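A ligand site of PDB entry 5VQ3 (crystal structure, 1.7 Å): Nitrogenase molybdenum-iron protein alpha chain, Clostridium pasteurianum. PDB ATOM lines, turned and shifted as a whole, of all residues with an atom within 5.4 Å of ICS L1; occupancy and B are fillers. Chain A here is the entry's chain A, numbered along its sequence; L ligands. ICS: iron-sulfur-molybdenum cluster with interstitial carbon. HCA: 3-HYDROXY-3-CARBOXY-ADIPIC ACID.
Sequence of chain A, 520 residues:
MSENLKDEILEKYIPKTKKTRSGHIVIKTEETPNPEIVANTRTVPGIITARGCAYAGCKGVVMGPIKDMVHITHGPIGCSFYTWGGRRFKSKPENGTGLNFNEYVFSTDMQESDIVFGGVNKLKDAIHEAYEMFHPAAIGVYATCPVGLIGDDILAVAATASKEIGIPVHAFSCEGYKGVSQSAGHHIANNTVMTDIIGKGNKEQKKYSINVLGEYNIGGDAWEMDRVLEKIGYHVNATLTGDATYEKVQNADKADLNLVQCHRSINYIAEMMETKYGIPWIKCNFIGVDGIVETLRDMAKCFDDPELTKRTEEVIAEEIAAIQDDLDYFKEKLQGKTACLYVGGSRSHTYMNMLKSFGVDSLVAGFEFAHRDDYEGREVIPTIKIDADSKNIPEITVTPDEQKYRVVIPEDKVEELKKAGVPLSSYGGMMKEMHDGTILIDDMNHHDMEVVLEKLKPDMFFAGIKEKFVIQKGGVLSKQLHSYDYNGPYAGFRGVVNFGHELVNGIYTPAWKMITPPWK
An oxygen (O7) of HCA L2 is bound to a molybdenum atom (MO1) of ICS L1, at 2.1 Å.
SG of Cys 262 lies close to OG of Ser 265 (3.2 Å). The backbone NH of Arg 264 lies close to the side-chain sulfur of Cys 262 (3.7 Å). NH1 of Arg 347 lies within hydrogen-bond range of O of His 482, 3.1 Å away. The guanidinium group (NH2) of Arg 87 is in hydrogen-bond range of the backbone carbonyl oxygen (O) of Val 61 (2.8 Å). N of Phe 369 is in hydrogen-bond range of O of Gly 344 (3.1 Å). NH1 of Arg 347 sits close to O of Leu 481, at 3.3 Å. The side-chain hydroxyl (OG) of Ser 265 is in hydrogen-bond range of the side-chain hydroxyl (OH) of Tyr 216 (2.7 Å). The backbone carbonyl oxygen (O) of Val 343 sits at hydrogen-bond distance from the backbone NH (N) of Glu 368, 2.9 Å away.
SG of Cys 262 is bound to FE1 of ICS L1, at 2.3 Å. ND1 of His 482 is bound to MO1 of ICS L1. A sulfur (S2B) of ICS L1 sits close to a ring nitrogen (NE2) of His 186 (3.2 Å). The guanidinium group of Arg 87 lies close to a sulfur (S5A) of ICS L1 (3.3 Å). S3A of ICS L1 lies close to N of Arg 347. The guanidinium group (NH2) of Arg 347 sits close to a sulfur (S5A) of ICS L1. The backbone NH (N) of Gly 344 sits close to a sulfur (S3A) of ICS L1, at 3.4 Å. N of Gly 345 lies close to S3A of ICS L1, at 3.5 Å. A sulfur (S2A) of ICS L1 lies close to the side-chain hydroxyl (OG) of Ser 265, at 3.6 Å. N of Ser 346 sits close to S3A of ICS L1. NE2 of Gln 182 sits at hydrogen-bond distance from O2 of HCA L2 (2.9 Å).
Residues that only touch ICS L1: Val 61 (3.5 Å), Tyr 216 (3.5 Å), Val 343 (3.96 Å) and Phe 369 (3.3 Å). Hydrophobic or aromatic side chains that line ICS L1: Val 61, His 186, Tyr 216, Val 343, Phe 369 and His 482. Of the 18 residues printed, 13 come within 4 Å of ICS L1. Along chain A the residues within 4 Å of ICS L1 span positions 61 to 482.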
ATOM      1  N   VAL A  61      12.920  -1.284  22.639  1.00  0.00           N
ATOM      2  CA  VAL A  61      12.459  -2.668  22.544  1.00  0.00           C
ATOM      3  C   VAL A  61      11.617  -2.939  21.303  1.00  0.00           C
ATOM      4  O   VAL A  61      12.026  -3.683  20.438  1.00  0.00           O
ATOM      5  CB  VAL A  61      11.722  -3.089  23.817  1.00  0.00           C
ATOM      6  CG1 VAL A  61      11.093  -4.472  23.666  1.00  0.00           C
ATOM      7  CG2 VAL A  61      12.687  -3.044  24.988  1.00  0.00           C
ATOM      8  N   ARG A  87      21.089  -3.651  23.227  1.00  0.00           N
ATOM      9  CA  ARG A  87      20.119  -4.698  22.949  1.00  0.00           C
ATOM     10  C   ARG A  87      20.374  -5.297  21.560  1.00  0.00           C
ATOM     11  O   ARG A  87      20.445  -4.612  20.539  1.00  0.00           O
ATOM     12  CB  ARG A  87      18.683  -4.163  23.089  1.00  0.00           C
ATOM     13  CG  ARG A  87      17.620  -5.221  22.856  1.00  0.00           C
ATOM     14  CD  ARG A  87      16.277  -4.763  23.430  1.00  0.00           C
ATOM     15  NE  ARG A  87      15.190  -5.671  23.036  1.00  0.00           N
ATOM     16  CZ  ARG A  87      14.437  -5.566  21.932  1.00  0.00           C
ATOM     17  NH1 ARG A  87      13.438  -6.420  21.759  1.00  0.00           N
ATOM     18  NH2 ARG A  87      14.610  -4.605  21.053  1.00  0.00           N
ATOM     19  N   GLN A 182       8.989  -0.815  31.502  1.00  0.00           N
ATOM     20  CA  GLN A 182       9.051  -0.914  30.053  1.00  0.00           C
ATOM     21  C   GLN A 182       7.722  -1.262  29.417  1.00  0.00           C
ATOM     22  O   GLN A 182       7.477  -0.921  28.286  1.00  0.00           O
ATOM     23  CB  GLN A 182      10.049  -2.013  29.648  1.00  0.00           C
ATOM     24  CG  GLN A 182      11.513  -1.785  30.021  1.00  0.00           C
ATOM     25  CD  GLN A 182      11.907  -2.372  31.326  1.00  0.00           C
ATOM     26  OE1 GLN A 182      11.208  -2.235  32.344  1.00  0.00           O
ATOM     27  NE2 GLN A 182      13.056  -3.021  31.338  1.00  0.00           N
ATOM     28  N   HIS A 186       5.685  -0.696  25.548  1.00  0.00           N
ATOM     29  CA  HIS A 186       5.196  -1.686  24.566  1.00  0.00           C
ATOM     30  C   HIS A 186       3.826  -1.224  24.054  1.00  0.00           C
ATOM     31  O   HIS A 186       3.546  -1.207  22.859  1.00  0.00           O
ATOM     32  CB  HIS A 186       5.034  -3.086  25.198  1.00  0.00           C
ATOM     33  CG  HIS A 186       6.268  -3.647  25.806  1.00  0.00           C
ATOM     34  ND1 HIS A 186       6.226  -4.574  26.833  1.00  0.00           N
ATOM     35  CD2 HIS A 186       7.578  -3.451  25.545  1.00  0.00           C
ATOM     36  CE1 HIS A 186       7.447  -4.951  27.137  1.00  0.00           C
ATOM     37  NE2 HIS A 186       8.294  -4.257  26.397  1.00  0.00           N
ATOM     38  N   TYR A 216      12.227 -10.446  18.424  1.00  0.00           N
ATOM     39  CA  TYR A 216      13.085  -9.275  18.107  1.00  0.00           C
ATOM     40  C   TYR A 216      14.439  -9.670  17.587  1.00  0.00           C
ATOM     41  O   TYR A 216      15.321  -8.810  17.396  1.00  0.00           O
ATOM     42  CB  TYR A 216      13.148  -8.345  19.334  1.00  0.00           C
ATOM     43  CG  TYR A 216      11.730  -7.965  19.765  1.00  0.00           C
ATOM     44  CD1 TYR A 216      10.989  -7.013  19.041  1.00  0.00           C
ATOM     45  CD2 TYR A 216      11.100  -8.599  20.841  1.00  0.00           C
ATOM     46  CE1 TYR A 216       9.690  -6.696  19.399  1.00  0.00           C
ATOM     47  CE2 TYR A 216       9.789  -8.289  21.172  1.00  0.00           C
ATOM     48  CZ  TYR A 216       9.096  -7.320  20.455  1.00  0.00           C
ATOM     49  OH  TYR A 216       7.777  -6.988  20.744  1.00  0.00           O
ATOM     50  N   ILE A 218      16.939 -11.315  18.739  1.00  0.00           N
ATOM     51  CA  ILE A 218      18.090 -11.149  19.641  1.00  0.00           C
ATOM     52  C   ILE A 218      19.077 -12.268  19.347  1.00  0.00           C
ATOM     53  O   ILE A 218      18.717 -13.452  19.323  1.00  0.00           O
ATOM     54  CB  ILE A 218      17.701 -11.176  21.104  1.00  0.00           C
ATOM     55  CG1 ILE A 218      16.576 -10.164  21.400  1.00  0.00           C
ATOM     56  CG2 ILE A 218      18.906 -10.926  21.986  1.00  0.00           C
ATOM     57  CD1 ILE A 218      16.874  -8.723  20.951  1.00  0.00           C
ATOM     58  N   CYS A 262       6.453 -13.315  22.471  1.00  0.00           N
ATOM     59  CA  CYS A 262       6.366 -12.503  23.702  1.00  0.00           C
ATOM     60  C   CYS A 262       4.957 -11.969  23.873  1.00  0.00           C
ATOM     61  O   CYS A 262       4.554 -10.999  23.201  1.00  0.00           O
ATOM     62  CB  CYS A 262       7.320 -11.314  23.677  1.00  0.00           C
ATOM     63  SG  CYS A 262       7.092 -10.347  25.193  1.00  0.00           S
ATOM     64  N   ARG A 264       3.636 -10.397  26.560  1.00  0.00           N
ATOM     65  CA  ARG A 264       3.630  -9.111  27.193  1.00  0.00           C
ATOM     66  C   ARG A 264       3.707  -7.959  26.191  1.00  0.00           C
ATOM     67  O   ARG A 264       2.920  -7.024  26.225  1.00  0.00           O
ATOM     68  CB  ARG A 264       4.766  -9.054  28.223  1.00  0.00           C
ATOM     69  CG  ARG A 264       4.830  -7.805  29.093  1.00  0.00           C
ATOM     70  CD  ARG A 264       3.584  -7.572  29.977  1.00  0.00           C
ATOM     71  NE  ARG A 264       2.504  -6.835  29.290  1.00  0.00           N
ATOM     72  CZ  ARG A 264       1.228  -7.266  29.180  1.00  0.00           C
ATOM     73  NH1 ARG A 264       0.811  -8.413  29.729  1.00  0.00           N
ATOM     74  NH2 ARG A 264       0.356  -6.498  28.532  1.00  0.00           N
ATOM     75  N   SER A 265       4.670  -8.026  25.274  1.00  0.00           N
ATOM     76  CA  SER A 265       4.990  -6.862  24.505  1.00  0.00           C
ATOM     77  C   SER A 265       4.096  -6.712  23.295  1.00  0.00           C
ATOM     78  O   SER A 265       4.027  -5.618  22.754  1.00  0.00           O
ATOM     79  CB  SER A 265       6.459  -6.862  23.997  1.00  0.00           C
ATOM     80  OG  SER A 265       6.681  -7.924  23.078  1.00  0.00           O
ATOM     81  N   VAL A 343      13.915 -12.536  34.727  1.00  0.00           N
ATOM     82  CA  VAL A 343      13.861 -11.830  33.468  1.00  0.00           C
ATOM     83  C   VAL A 343      12.917 -10.657  33.502  1.00  0.00           C
ATOM     84  O   VAL A 343      12.412 -10.262  34.571  1.00  0.00           O
ATOM     85  CB  VAL A 343      13.462 -12.737  32.341  1.00  0.00           C
ATOM     86  CG1 VAL A 343      14.357 -13.991  32.347  1.00  0.00           C
ATOM     87  CG2 VAL A 343      11.988 -13.043  32.451  1.00  0.00           C
ATOM     88  N   GLY A 344      12.670 -10.100  32.321  1.00  0.00           N
ATOM     89  CA  GLY A 344      11.836  -8.944  32.208  1.00  0.00           C
ATOM     90  C   GLY A 344      10.367  -9.245  32.340  1.00  0.00           C
ATOM     91  O   GLY A 344       9.743  -8.974  33.373  1.00  0.00           O
ATOM     92  N   GLY A 345       9.796  -9.754  31.245  1.00  0.00           N
ATOM     93  CA  GLY A 345       8.383  -9.954  31.189  1.00  0.00           C
ATOM     94  C   GLY A 345       7.925 -11.233  30.540  1.00  0.00           C
ATOM     95  O   GLY A 345       6.714 -11.439  30.442  1.00  0.00           O
ATOM     96  N   SER A 346       8.884 -12.070  30.132  1.00  0.00           N
ATOM     97  CA  SER A 346       8.627 -13.307  29.375  1.00  0.00           C
ATOM     98  C   SER A 346       9.725 -14.412  29.499  1.00  0.00           C
ATOM     99  O   SER A 346       9.405 -15.602  29.674  1.00  0.00           O
ATOM    100  CB  SER A 346       8.384 -12.944  27.893  1.00  0.00           C
ATOM    101  OG  SER A 346       8.511 -14.070  27.021  1.00  0.00           O
ATOM    102  N   ARG A 347      10.990 -14.055  29.449  1.00  0.00           N
ATOM    103  CA  ARG A 347      12.017 -15.127  29.366  1.00  0.00           C
ATOM    104  C   ARG A 347      12.237 -15.960  30.612  1.00  0.00           C
ATOM    105  O   ARG A 347      12.935 -16.932  30.600  1.00  0.00           O
ATOM    106  CB  ARG A 347      13.373 -14.655  28.817  1.00  0.00           C
ATOM    107  CG  ARG A 347      13.323 -13.992  27.444  1.00  0.00           C
ATOM    108  CD  ARG A 347      14.687 -13.635  26.881  1.00  0.00           C
ATOM    109  NE  ARG A 347      14.382 -13.066  25.543  1.00  0.00           N
ATOM    110  CZ  ARG A 347      15.197 -12.461  24.681  1.00  0.00           C
ATOM    111  NH1 ARG A 347      16.464 -12.151  24.957  1.00  0.00           N
ATOM    112  NH2 ARG A 347      14.686 -12.092  23.530  1.00  0.00           N
ATOM    113  N   GLU A 368      10.726  -8.566  36.187  1.00  0.00           N
ATOM    114  CA  GLU A 368      10.715  -7.132  36.438  1.00  0.00           C
ATOM    115  C   GLU A 368       9.301  -6.550  36.340  1.00  0.00           C
ATOM    116  O   GLU A 368       8.913  -5.727  37.177  1.00  0.00           O
ATOM    117  CB  GLU A 368      11.583  -6.383  35.444  1.00  0.00           C
ATOM    118  CG  GLU A 368      13.051  -6.728  35.465  1.00  0.00           C
ATOM    119  CD  GLU A 368      13.898  -5.999  34.387  1.00  0.00           C
ATOM    120  OE1 GLU A 368      15.071  -6.448  34.152  1.00  0.00           O
ATOM    121  OE2 GLU A 368      13.432  -4.974  33.822  1.00  0.00           O
ATOM    122  N   PHE A 369       8.571  -6.868  35.261  1.00  0.00           N
ATOM    123  CA  PHE A 369       7.390  -6.030  34.879  1.00  0.00           C
ATOM    124  C   PHE A 369       6.209  -6.762  34.242  1.00  0.00           C
ATOM    125  O   PHE A 369       5.306  -6.088  33.703  1.00  0.00           O
ATOM    126  CB  PHE A 369       7.848  -4.873  33.948  1.00  0.00           C
ATOM    127  CG  PHE A 369       8.556  -5.331  32.704  1.00  0.00           C
ATOM    128  CD1 PHE A 369       7.852  -6.019  31.713  1.00  0.00           C
ATOM    129  CD2 PHE A 369       9.901  -5.179  32.563  1.00  0.00           C
ATOM    130  CE1 PHE A 369       8.512  -6.488  30.598  1.00  0.00           C
ATOM    131  CE2 PHE A 369      10.576  -5.665  31.452  1.00  0.00           C
ATOM    132  CZ  PHE A 369       9.882  -6.327  30.485  1.00  0.00           C
ATOM    133  N   LEU A 481      20.151 -13.731  30.421  1.00  0.00           N
ATOM    134  CA  LEU A 481      19.022 -14.116  29.591  1.00  0.00           C
ATOM    135  C   LEU A 481      18.525 -13.024  28.664  1.00  0.00           C
ATOM    136  O   LEU A 481      17.657 -13.264  27.849  1.00  0.00           O
ATOM    137  CB  LEU A 481      17.879 -14.656  30.451  1.00  0.00           C
ATOM    138  CG  LEU A 481      18.184 -16.023  31.084  1.00  0.00           C
ATOM    139  CD1 LEU A 481      17.015 -16.465  31.938  1.00  0.00           C
ATOM    140  CD2 LEU A 481      18.488 -17.039  29.996  1.00  0.00           C
ATOM    141  N   HIS A 482      19.040 -11.796  28.771  1.00  0.00           N
ATOM    142  CA  HIS A 482      18.670 -10.784  27.783  1.00  0.00           C
ATOM    143  C   HIS A 482      19.699 -10.757  26.630  1.00  0.00           C
ATOM    144  O   HIS A 482      19.335 -11.008  25.480  1.00  0.00           O
ATOM    145  CB  HIS A 482      18.601  -9.371  28.365  1.00  0.00           C
ATOM    146  CG  HIS A 482      17.804  -9.239  29.621  1.00  0.00           C
ATOM    147  ND1 HIS A 482      16.674  -8.443  29.713  1.00  0.00           N
ATOM    148  CD2 HIS A 482      18.070  -9.642  30.889  1.00  0.00           C
ATOM    149  CE1 HIS A 482      16.244  -8.447  30.959  1.00  0.00           C
ATOM    150  NE2 HIS A 482      17.077  -9.170  31.697  1.00  0.00           N
HETATM  151 FE1  ICS L   1       9.159  -9.510  25.712  1.00  0.00          FE
HETATM  152 MO1  ICS L   1      15.410  -7.387  28.012  1.00  0.00          MO
HETATM  153 FE2  ICS L   1      10.528  -7.457  26.745  1.00  0.00          FE
HETATM  154 FE3  ICS L   1      11.728  -9.081  24.990  1.00  0.00          FE
HETATM  155 FE4  ICS L   1      11.097  -9.962  27.443  1.00  0.00          FE
HETATM  156 FE5  ICS L   1      13.398  -9.145  28.295  1.00  0.00          FE
HETATM  157 FE6  ICS L   1      12.842  -6.682  27.584  1.00  0.00          FE
HETATM  158 FE7  ICS L   1      14.021  -8.292  25.912  1.00  0.00          FE
HETATM  159  CX  ICS L   1      12.255  -8.494  26.854  1.00  0.00           C
HETATM  160  S1A ICS L   1       9.147  -8.850  27.880  1.00  0.00           S
HETATM  161  S1B ICS L   1      13.630  -7.285  29.559  1.00  0.00           S
HETATM  162  S2A ICS L   1       9.936  -7.684  24.612  1.00  0.00           S
HETATM  163  S2B ICS L   1      11.059  -5.427  27.515  1.00  0.00           S
HETATM  164  S3A ICS L   1      12.240 -10.872  29.071  1.00  0.00           S
HETATM  165  S3B ICS L   1      14.482  -6.135  26.226  1.00  0.00           S
HETATM  166  S4A ICS L   1      10.820 -11.095  25.480  1.00  0.00           S
HETATM  167  S4B ICS L   1      15.309  -9.586  27.184  1.00  0.00           S
HETATM  168  S5A ICS L   1      13.643  -8.954  23.843  1.00  0.00           S
HETATM  169  C1  HCA L   2      15.793  -2.863  28.508  1.00  0.00           C
HETATM  170  C2  HCA L   2      16.741  -3.619  27.593  1.00  0.00           C
HETATM  171  C3  HCA L   2      17.248  -4.907  28.255  1.00  0.00           C
HETATM  172  C4  HCA L   2      18.366  -4.709  29.286  1.00  0.00           C
HETATM  173  C5  HCA L   2      19.072  -6.050  29.569  1.00  0.00           C
HETATM  174  C6  HCA L   2      19.844  -6.227  30.869  1.00  0.00           C
HETATM  175  C7  HCA L   2      17.788  -5.806  27.155  1.00  0.00           C
HETATM  176  O1  HCA L   2      15.697  -1.609  28.368  1.00  0.00           O
HETATM  177  O2  HCA L   2      15.182  -3.499  29.363  1.00  0.00           O
HETATM  178  O3  HCA L   2      20.865  -6.989  30.849  1.00  0.00           O
HETATM  179  O4  HCA L   2      19.434  -5.680  31.930  1.00  0.00           O
HETATM  180  O5  HCA L   2      18.709  -5.370  26.413  1.00  0.00           O
HETATM  181  O6  HCA L   2      17.340  -6.982  27.014  1.00  0.00           O
HETATM  182  O7  HCA L   2      16.134  -5.582  28.883  1.00  0.00           O
